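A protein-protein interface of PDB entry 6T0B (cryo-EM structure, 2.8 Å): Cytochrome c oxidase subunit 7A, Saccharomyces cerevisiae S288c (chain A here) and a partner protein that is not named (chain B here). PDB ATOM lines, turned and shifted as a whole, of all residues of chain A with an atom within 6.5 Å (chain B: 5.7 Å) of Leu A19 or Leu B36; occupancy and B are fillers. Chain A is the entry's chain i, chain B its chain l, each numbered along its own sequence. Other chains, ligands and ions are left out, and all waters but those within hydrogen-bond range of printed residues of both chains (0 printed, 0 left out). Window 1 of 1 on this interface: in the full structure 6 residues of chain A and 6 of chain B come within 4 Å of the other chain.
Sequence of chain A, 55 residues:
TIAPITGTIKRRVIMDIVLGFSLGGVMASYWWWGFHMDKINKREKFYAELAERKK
The guanidinium group of Arg A12 lies within salt-bridge range of the side-chain carboxylate of Glu B32 (3.9 Å).
Among the printed residues, merely in contact across the chains: Leu A19 with Ile B40 (3.8 Å), Asp A16 with Leu B36 (3.9 Å) and Leu A19 with Leu B36 (3.95 Å).
Leu A19 touches just these residues of chain B: Leu B36 and Ile B40. Leu B36 touches two residues of chain A. Printed residues of chain B within 4 Å of Arg A12: Glu B32 (3.9 Å). Of the printed residues of chain B, Asp A16 touches Leu B36. Printed residues of chain A within 4 Å of Glu B32: Arg A12. Of the printed residues of chain A, Ile B40 touches Leu A19. The nearest printed residue of chain B that does not touch Leu A19 is Ile B37 (6.6 Å). The nearest residue of chain A that does not touch Leu B36 is Met A15 (4.9 Å).
Of the 10 printed residues of chain B, 3 touch a printed residue of chain A. Hydrophobic or aromatic side chains of chain B that line the printed part of chain A: Leu B36 and Ile B40. Hydrophobic or aromatic side chains of chain A within 4 Å of the printed part of chain B: Leu A19. Along chain A the printed residues that touch a printed residue of chain B span positions 12 to 19. Among the printed residues, 4 pairs touch across the chains.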
ATOM      1  N   ARG A  12     -37.982 -20.860 -17.787  1.00  0.00           N
ATOM      2  CA  ARG A  12     -36.886 -21.191 -18.683  1.00  0.00           C
ATOM      3  C   ARG A  12     -36.908 -20.335 -19.942  1.00  0.00           C
ATOM      4  O   ARG A  12     -35.870 -19.815 -20.356  1.00  0.00           O
ATOM      5  CB  ARG A  12     -36.947 -22.668 -19.035  1.00  0.00           C
ATOM      6  CG  ARG A  12     -35.763 -23.169 -19.772  1.00  0.00           C
ATOM      7  CD  ARG A  12     -35.812 -24.668 -19.866  1.00  0.00           C
ATOM      8  NE  ARG A  12     -35.396 -25.306 -18.631  1.00  0.00           N
ATOM      9  CZ  ARG A  12     -35.148 -26.602 -18.517  1.00  0.00           C
ATOM     10  NH1 ARG A  12     -35.279 -27.394 -19.565  1.00  0.00           N
ATOM     11  NH2 ARG A  12     -34.768 -27.108 -17.355  1.00  0.00           N
ATOM     12  N   ILE A  14     -38.346 -17.482 -20.110  1.00  0.00           N
ATOM     13  CA  ILE A  14     -38.173 -16.095 -19.701  1.00  0.00           C
ATOM     14  C   ILE A  14     -36.691 -15.769 -19.550  1.00  0.00           C
ATOM     15  O   ILE A  14     -36.205 -14.762 -20.088  1.00  0.00           O
ATOM     16  CB  ILE A  14     -38.968 -15.819 -18.418  1.00  0.00           C
ATOM     17  CG1 ILE A  14     -40.438 -15.624 -18.764  1.00  0.00           C
ATOM     18  CG2 ILE A  14     -38.468 -14.591 -17.720  1.00  0.00           C
ATOM     19  CD1 ILE A  14     -41.334 -15.538 -17.572  1.00  0.00           C
ATOM     20  N   MET A  15     -35.932 -16.659 -18.897  1.00  0.00           N
ATOM     21  CA  MET A  15     -34.497 -16.425 -18.789  1.00  0.00           C
ATOM     22  C   MET A  15     -33.790 -16.594 -20.125  1.00  0.00           C
ATOM     23  O   MET A  15     -32.811 -15.895 -20.382  1.00  0.00           O
ATOM     24  CB  MET A  15     -33.879 -17.336 -17.739  1.00  0.00           C
ATOM     25  CG  MET A  15     -34.437 -17.112 -16.341  1.00  0.00           C
ATOM     26  SD  MET A  15     -34.450 -15.382 -15.823  1.00  0.00           S
ATOM     27  CE  MET A  15     -36.020 -15.275 -14.963  1.00  0.00           C
ATOM     28  N   ASP A  16     -34.304 -17.445 -21.016  1.00  0.00           N
ATOM     29  CA  ASP A  16     -33.686 -17.597 -22.329  1.00  0.00           C
ATOM     30  C   ASP A  16     -33.877 -16.363 -23.189  1.00  0.00           C
ATOM     31  O   ASP A  16     -32.950 -15.937 -23.876  1.00  0.00           O
ATOM     32  CB  ASP A  16     -34.254 -18.814 -23.047  1.00  0.00           C
ATOM     33  CG  ASP A  16     -33.604 -20.093 -22.613  1.00  0.00           C
ATOM     34  OD1 ASP A  16     -32.424 -20.054 -22.221  1.00  0.00           O
ATOM     35  OD2 ASP A  16     -34.272 -21.144 -22.648  1.00  0.00           O
ATOM     36  N   ILE A  17     -35.061 -15.766 -23.152  1.00  0.00           N
ATOM     37  CA  ILE A  17     -35.312 -14.574 -23.948  1.00  0.00           C
ATOM     38  C   ILE A  17     -34.543 -13.383 -23.386  1.00  0.00           C
ATOM     39  O   ILE A  17     -33.965 -12.588 -24.145  1.00  0.00           O
ATOM     40  CB  ILE A  17     -36.827 -14.323 -24.023  1.00  0.00           C
ATOM     41  CG1 ILE A  17     -37.477 -15.372 -24.910  1.00  0.00           C
ATOM     42  CG2 ILE A  17     -37.142 -12.973 -24.588  1.00  0.00           C
ATOM     43  CD1 ILE A  17     -38.960 -15.334 -24.867  1.00  0.00           C
ATOM     44  N   VAL A  18     -34.472 -13.271 -22.052  1.00  0.00           N
ATOM     45  CA  VAL A  18     -33.691 -12.206 -21.420  1.00  0.00           C
ATOM     46  C   VAL A  18     -32.209 -12.353 -21.746  1.00  0.00           C
ATOM     47  O   VAL A  18     -31.535 -11.376 -22.098  1.00  0.00           O
ATOM     48  CB  VAL A  18     -33.947 -12.205 -19.904  1.00  0.00           C
ATOM     49  CG1 VAL A  18     -32.864 -11.463 -19.161  1.00  0.00           C
ATOM     50  CG2 VAL A  18     -35.277 -11.585 -19.619  1.00  0.00           C
ATOM     51  N   LEU A  19     -31.697 -13.583 -21.697  1.00  0.00           N
ATOM     52  CA  LEU A  19     -30.302 -13.834 -22.024  1.00  0.00           C
ATOM     53  C   LEU A  19     -30.016 -13.578 -23.492  1.00  0.00           C
ATOM     54  O   LEU A  19     -28.940 -13.087 -23.835  1.00  0.00           O
ATOM     55  CB  LEU A  19     -29.946 -15.267 -21.663  1.00  0.00           C
ATOM     56  CG  LEU A  19     -28.481 -15.661 -21.680  1.00  0.00           C
ATOM     57  CD1 LEU A  19     -27.645 -14.626 -20.969  1.00  0.00           C
ATOM     58  CD2 LEU A  19     -28.340 -16.989 -20.995  1.00  0.00           C
ATOM     59  N   GLY A  20     -30.965 -13.890 -24.370  1.00  0.00           N
ATOM     60  CA  GLY A  20     -30.759 -13.634 -25.783  1.00  0.00           C
ATOM     61  C   GLY A  20     -30.711 -12.160 -26.097  1.00  0.00           C
ATOM     62  O   GLY A  20     -29.874 -11.714 -26.887  1.00  0.00           O
ATOM     63  N   PHE A  21     -31.574 -11.379 -25.453  1.00  0.00           N
ATOM     64  CA  PHE A  21     -31.526  -9.937 -25.642  1.00  0.00           C
ATOM     65  C   PHE A  21     -30.266  -9.340 -25.039  1.00  0.00           C
ATOM     66  O   PHE A  21     -29.704  -8.399 -25.599  1.00  0.00           O
ATOM     67  CB  PHE A  21     -32.765  -9.284 -25.056  1.00  0.00           C
ATOM     68  CG  PHE A  21     -33.931  -9.328 -25.967  1.00  0.00           C
ATOM     69  CD1 PHE A  21     -33.835  -8.810 -27.236  1.00  0.00           C
ATOM     70  CD2 PHE A  21     -35.115  -9.906 -25.574  1.00  0.00           C
ATOM     71  CE1 PHE A  21     -34.895  -8.858 -28.094  1.00  0.00           C
ATOM     72  CE2 PHE A  21     -36.183  -9.955 -26.431  1.00  0.00           C
ATOM     73  CZ  PHE A  21     -36.071  -9.426 -27.695  1.00  0.00           C
ATOM     74  N   SER A  22     -29.766  -9.909 -23.942  1.00  0.00           N
ATOM     75  CA  SER A  22     -28.552  -9.362 -23.345  1.00  0.00           C
ATOM     76  C   SER A  22     -27.310  -9.719 -24.151  1.00  0.00           C
ATOM     77  O   SER A  22     -26.382  -8.910 -24.254  1.00  0.00           O
ATOM     78  CB  SER A  22     -28.416  -9.841 -21.907  1.00  0.00           C
ATOM     79  OG  SER A  22     -29.461  -9.314 -21.114  1.00  0.00           O
ATOM     80  N   LEU A  23     -27.274 -10.908 -24.750  1.00  0.00           N
ATOM     81  CA  LEU A  23     -26.133 -11.264 -25.587  1.00  0.00           C
ATOM     82  C   LEU A  23     -26.146 -10.491 -26.898  1.00  0.00           C
ATOM     83  O   LEU A  23     -25.097 -10.021 -27.356  1.00  0.00           O
ATOM     84  CB  LEU A  23     -26.107 -12.765 -25.844  1.00  0.00           C
ATOM     85  CG  LEU A  23     -25.808 -13.581 -24.592  1.00  0.00           C
ATOM     86  CD1 LEU A  23     -25.911 -15.058 -24.878  1.00  0.00           C
ATOM     87  CD2 LEU A  23     -24.445 -13.234 -24.029  1.00  0.00           C
ATOM     88  N   GLY A  24     -27.323 -10.321 -27.503  1.00  0.00           N
ATOM     89  CA  GLY A  24     -27.423  -9.428 -28.639  1.00  0.00           C
ATOM     90  C   GLY A  24     -27.098  -7.994 -28.285  1.00  0.00           C
ATOM     91  O   GLY A  24     -26.516  -7.269 -29.095  1.00  0.00           O
ATOM     92  N   GLU B  32     -30.228 -23.576 -13.004  1.00  0.00           N
ATOM     93  CA  GLU B  32     -30.166 -23.163 -14.390  1.00  0.00           C
ATOM     94  C   GLU B  32     -28.925 -22.360 -14.724  1.00  0.00           C
ATOM     95  O   GLU B  32     -28.569 -22.290 -15.898  1.00  0.00           O
ATOM     96  CB  GLU B  32     -31.421 -22.369 -14.761  1.00  0.00           C
ATOM     97  CG  GLU B  32     -32.492 -23.252 -15.385  1.00  0.00           C
ATOM     98  CD  GLU B  32     -33.850 -22.601 -15.416  1.00  0.00           C
ATOM     99  OE1 GLU B  32     -33.912 -21.357 -15.511  1.00  0.00           O
ATOM    100  OE2 GLU B  32     -34.858 -23.334 -15.328  1.00  0.00           O
ATOM    101  N   GLY B  33     -28.233 -21.785 -13.741  1.00  0.00           N
ATOM    102  CA  GLY B  33     -26.949 -21.180 -14.027  1.00  0.00           C
ATOM    103  C   GLY B  33     -25.900 -22.211 -14.369  1.00  0.00           C
ATOM    104  O   GLY B  33     -25.149 -22.041 -15.332  1.00  0.00           O
ATOM    105  N   ARG B  34     -25.878 -23.328 -13.638  1.00  0.00           N
ATOM    106  CA  ARG B  34     -24.901 -24.364 -13.952  1.00  0.00           C
ATOM    107  C   ARG B  34     -25.208 -25.114 -15.245  1.00  0.00           C
ATOM    108  O   ARG B  34     -24.369 -25.898 -15.695  1.00  0.00           O
ATOM    109  CB  ARG B  34     -24.778 -25.347 -12.786  1.00  0.00           C
ATOM    110  CG  ARG B  34     -25.746 -26.503 -12.801  1.00  0.00           C
ATOM    111  CD  ARG B  34     -25.381 -27.489 -11.727  1.00  0.00           C
ATOM    112  NE  ARG B  34     -25.289 -26.827 -10.437  1.00  0.00           N
ATOM    113  CZ  ARG B  34     -24.434 -27.171  -9.487  1.00  0.00           C
ATOM    114  NH1 ARG B  34     -23.598 -28.178  -9.683  1.00  0.00           N
ATOM    115  NH2 ARG B  34     -24.417 -26.511  -8.343  1.00  0.00           N
ATOM    116  N   ARG B  35     -26.364 -24.884 -15.860  1.00  0.00           N
ATOM    117  CA  ARG B  35     -26.678 -25.384 -17.191  1.00  0.00           C
ATOM    118  C   ARG B  35     -26.453 -24.346 -18.284  1.00  0.00           C
ATOM    119  O   ARG B  35     -25.915 -24.672 -19.343  1.00  0.00           O
ATOM    120  CB  ARG B  35     -28.130 -25.862 -17.232  1.00  0.00           C
ATOM    121  CG  ARG B  35     -28.629 -26.274 -18.585  1.00  0.00           C
ATOM    122  CD  ARG B  35     -30.123 -26.449 -18.562  1.00  0.00           C
ATOM    123  NE  ARG B  35     -30.828 -25.176 -18.577  1.00  0.00           N
ATOM    124  CZ  ARG B  35     -31.117 -24.502 -19.683  1.00  0.00           C
ATOM    125  NH1 ARG B  35     -30.756 -24.977 -20.862  1.00  0.00           N
ATOM    126  NH2 ARG B  35     -31.766 -23.352 -19.611  1.00  0.00           N
ATOM    127  N   LEU B  36     -26.818 -23.094 -18.038  1.00  0.00           N
ATOM    128  CA  LEU B  36     -26.735 -22.057 -19.046  1.00  0.00           C
ATOM    129  C   LEU B  36     -25.359 -21.441 -19.182  1.00  0.00           C
ATOM    130  O   LEU B  36     -25.079 -20.846 -20.225  1.00  0.00           O
ATOM    131  CB  LEU B  36     -27.726 -20.942 -18.736  1.00  0.00           C
ATOM    132  CG  LEU B  36     -29.140 -21.159 -19.237  1.00  0.00           C
ATOM    133  CD1 LEU B  36     -29.961 -19.946 -18.929  1.00  0.00           C
ATOM    134  CD2 LEU B  36     -29.132 -21.431 -20.724  1.00  0.00           C
ATOM    135  N   ILE B  37     -24.505 -21.535 -18.169  1.00  0.00           N
ATOM    136  CA  ILE B  37     -23.172 -20.942 -18.258  1.00  0.00           C
ATOM    137  C   ILE B  37     -22.278 -21.614 -19.307  1.00  0.00           C
ATOM    138  O   ILE B  37     -21.695 -20.874 -20.108  1.00  0.00           O
ATOM    139  CB  ILE B  37     -22.512 -20.886 -16.868  1.00  0.00           C
ATOM    140  CG1 ILE B  37     -23.019 -19.670 -16.104  1.00  0.00           C
ATOM    141  CG2 ILE B  37     -21.009 -20.798 -16.952  1.00  0.00           C
ATOM    142  CD1 ILE B  37     -22.535 -19.606 -14.693  1.00  0.00           C
ATOM    143  N   PRO B  38     -22.136 -22.950 -19.407  1.00  0.00           N
ATOM    144  CA  PRO B  38     -21.269 -23.476 -20.477  1.00  0.00           C
ATOM    145  C   PRO B  38     -21.828 -23.295 -21.875  1.00  0.00           C
ATOM    146  O   PRO B  38     -21.050 -23.175 -22.830  1.00  0.00           O
ATOM    147  CB  PRO B  38     -21.141 -24.963 -20.132  1.00  0.00           C
ATOM    148  CG  PRO B  38     -21.538 -25.072 -18.750  1.00  0.00           C
ATOM    149  CD  PRO B  38     -22.594 -24.069 -18.566  1.00  0.00           C
ATOM    150  N   GLU B  39     -23.147 -23.256 -22.030  1.00  0.00           N
ATOM    151  CA  GLU B  39     -23.717 -23.096 -23.356  1.00  0.00           C
ATOM    152  C   GLU B  39     -23.575 -21.682 -23.885  1.00  0.00           C
ATOM    153  O   GLU B  39     -23.561 -21.503 -25.102  1.00  0.00           O
ATOM    154  CB  GLU B  39     -25.181 -23.521 -23.356  1.00  0.00           C
ATOM    155  CG  GLU B  39     -25.334 -25.013 -23.559  1.00  0.00           C
ATOM    156  CD  GLU B  39     -26.767 -25.468 -23.593  1.00  0.00           C
ATOM    157  OE1 GLU B  39     -26.995 -26.689 -23.522  1.00  0.00           O
ATOM    158  OE2 GLU B  39     -27.664 -24.615 -23.704  1.00  0.00           O
ATOM    159  N   ILE B  40     -23.429 -20.688 -23.005  1.00  0.00           N
ATOM    160  CA  ILE B  40     -23.065 -19.342 -23.438  1.00  0.00           C
ATOM    161  C   ILE B  40     -21.699 -19.355 -24.111  1.00  0.00           C
ATOM    162  O   ILE B  40     -21.512 -18.789 -25.194  1.00  0.00           O
ATOM    163  CB  ILE B  40     -23.087 -18.376 -22.242  1.00  0.00           C
ATOM    164  CG1 ILE B  40     -24.514 -18.019 -21.865  1.00  0.00           C
ATOM    165  CG2 ILE B  40     -22.345 -17.110 -22.554  1.00  0.00           C
ATOM    166  CD1 ILE B  40     -24.604 -17.220 -20.595  1.00  0.00           C
ATOM    167  N   PHE B  41     -20.736 -20.035 -23.493  1.00  0.00           N
ATOM    168  CA  PHE B  41     -19.389 -20.090 -24.045  1.00  0.00           C
ATOM    169  C   PHE B  41     -19.348 -20.909 -25.325  1.00  0.00           C
ATOM    170  O   PHE B  41     -18.623 -20.563 -26.270  1.00  0.00           O
ATOM    171  CB  PHE B  41     -18.431 -20.668 -23.009  1.00  0.00           C
ATOM    172  CG  PHE B  41     -18.076 -19.708 -21.919  1.00  0.00           C
ATOM    173  CD1 PHE B  41     -18.886 -19.570 -20.814  1.00  0.00           C
ATOM    174  CD2 PHE B  41     -16.933 -18.946 -21.999  1.00  0.00           C
ATOM    175  CE1 PHE B  41     -18.571 -18.686 -19.813  1.00  0.00           C
ATOM    176  CE2 PHE B  41     -16.610 -18.060 -20.996  1.00  0.00           C
ATOM    177  CZ  PHE B  41     -17.432 -17.933 -19.903  1.00  0.00           C
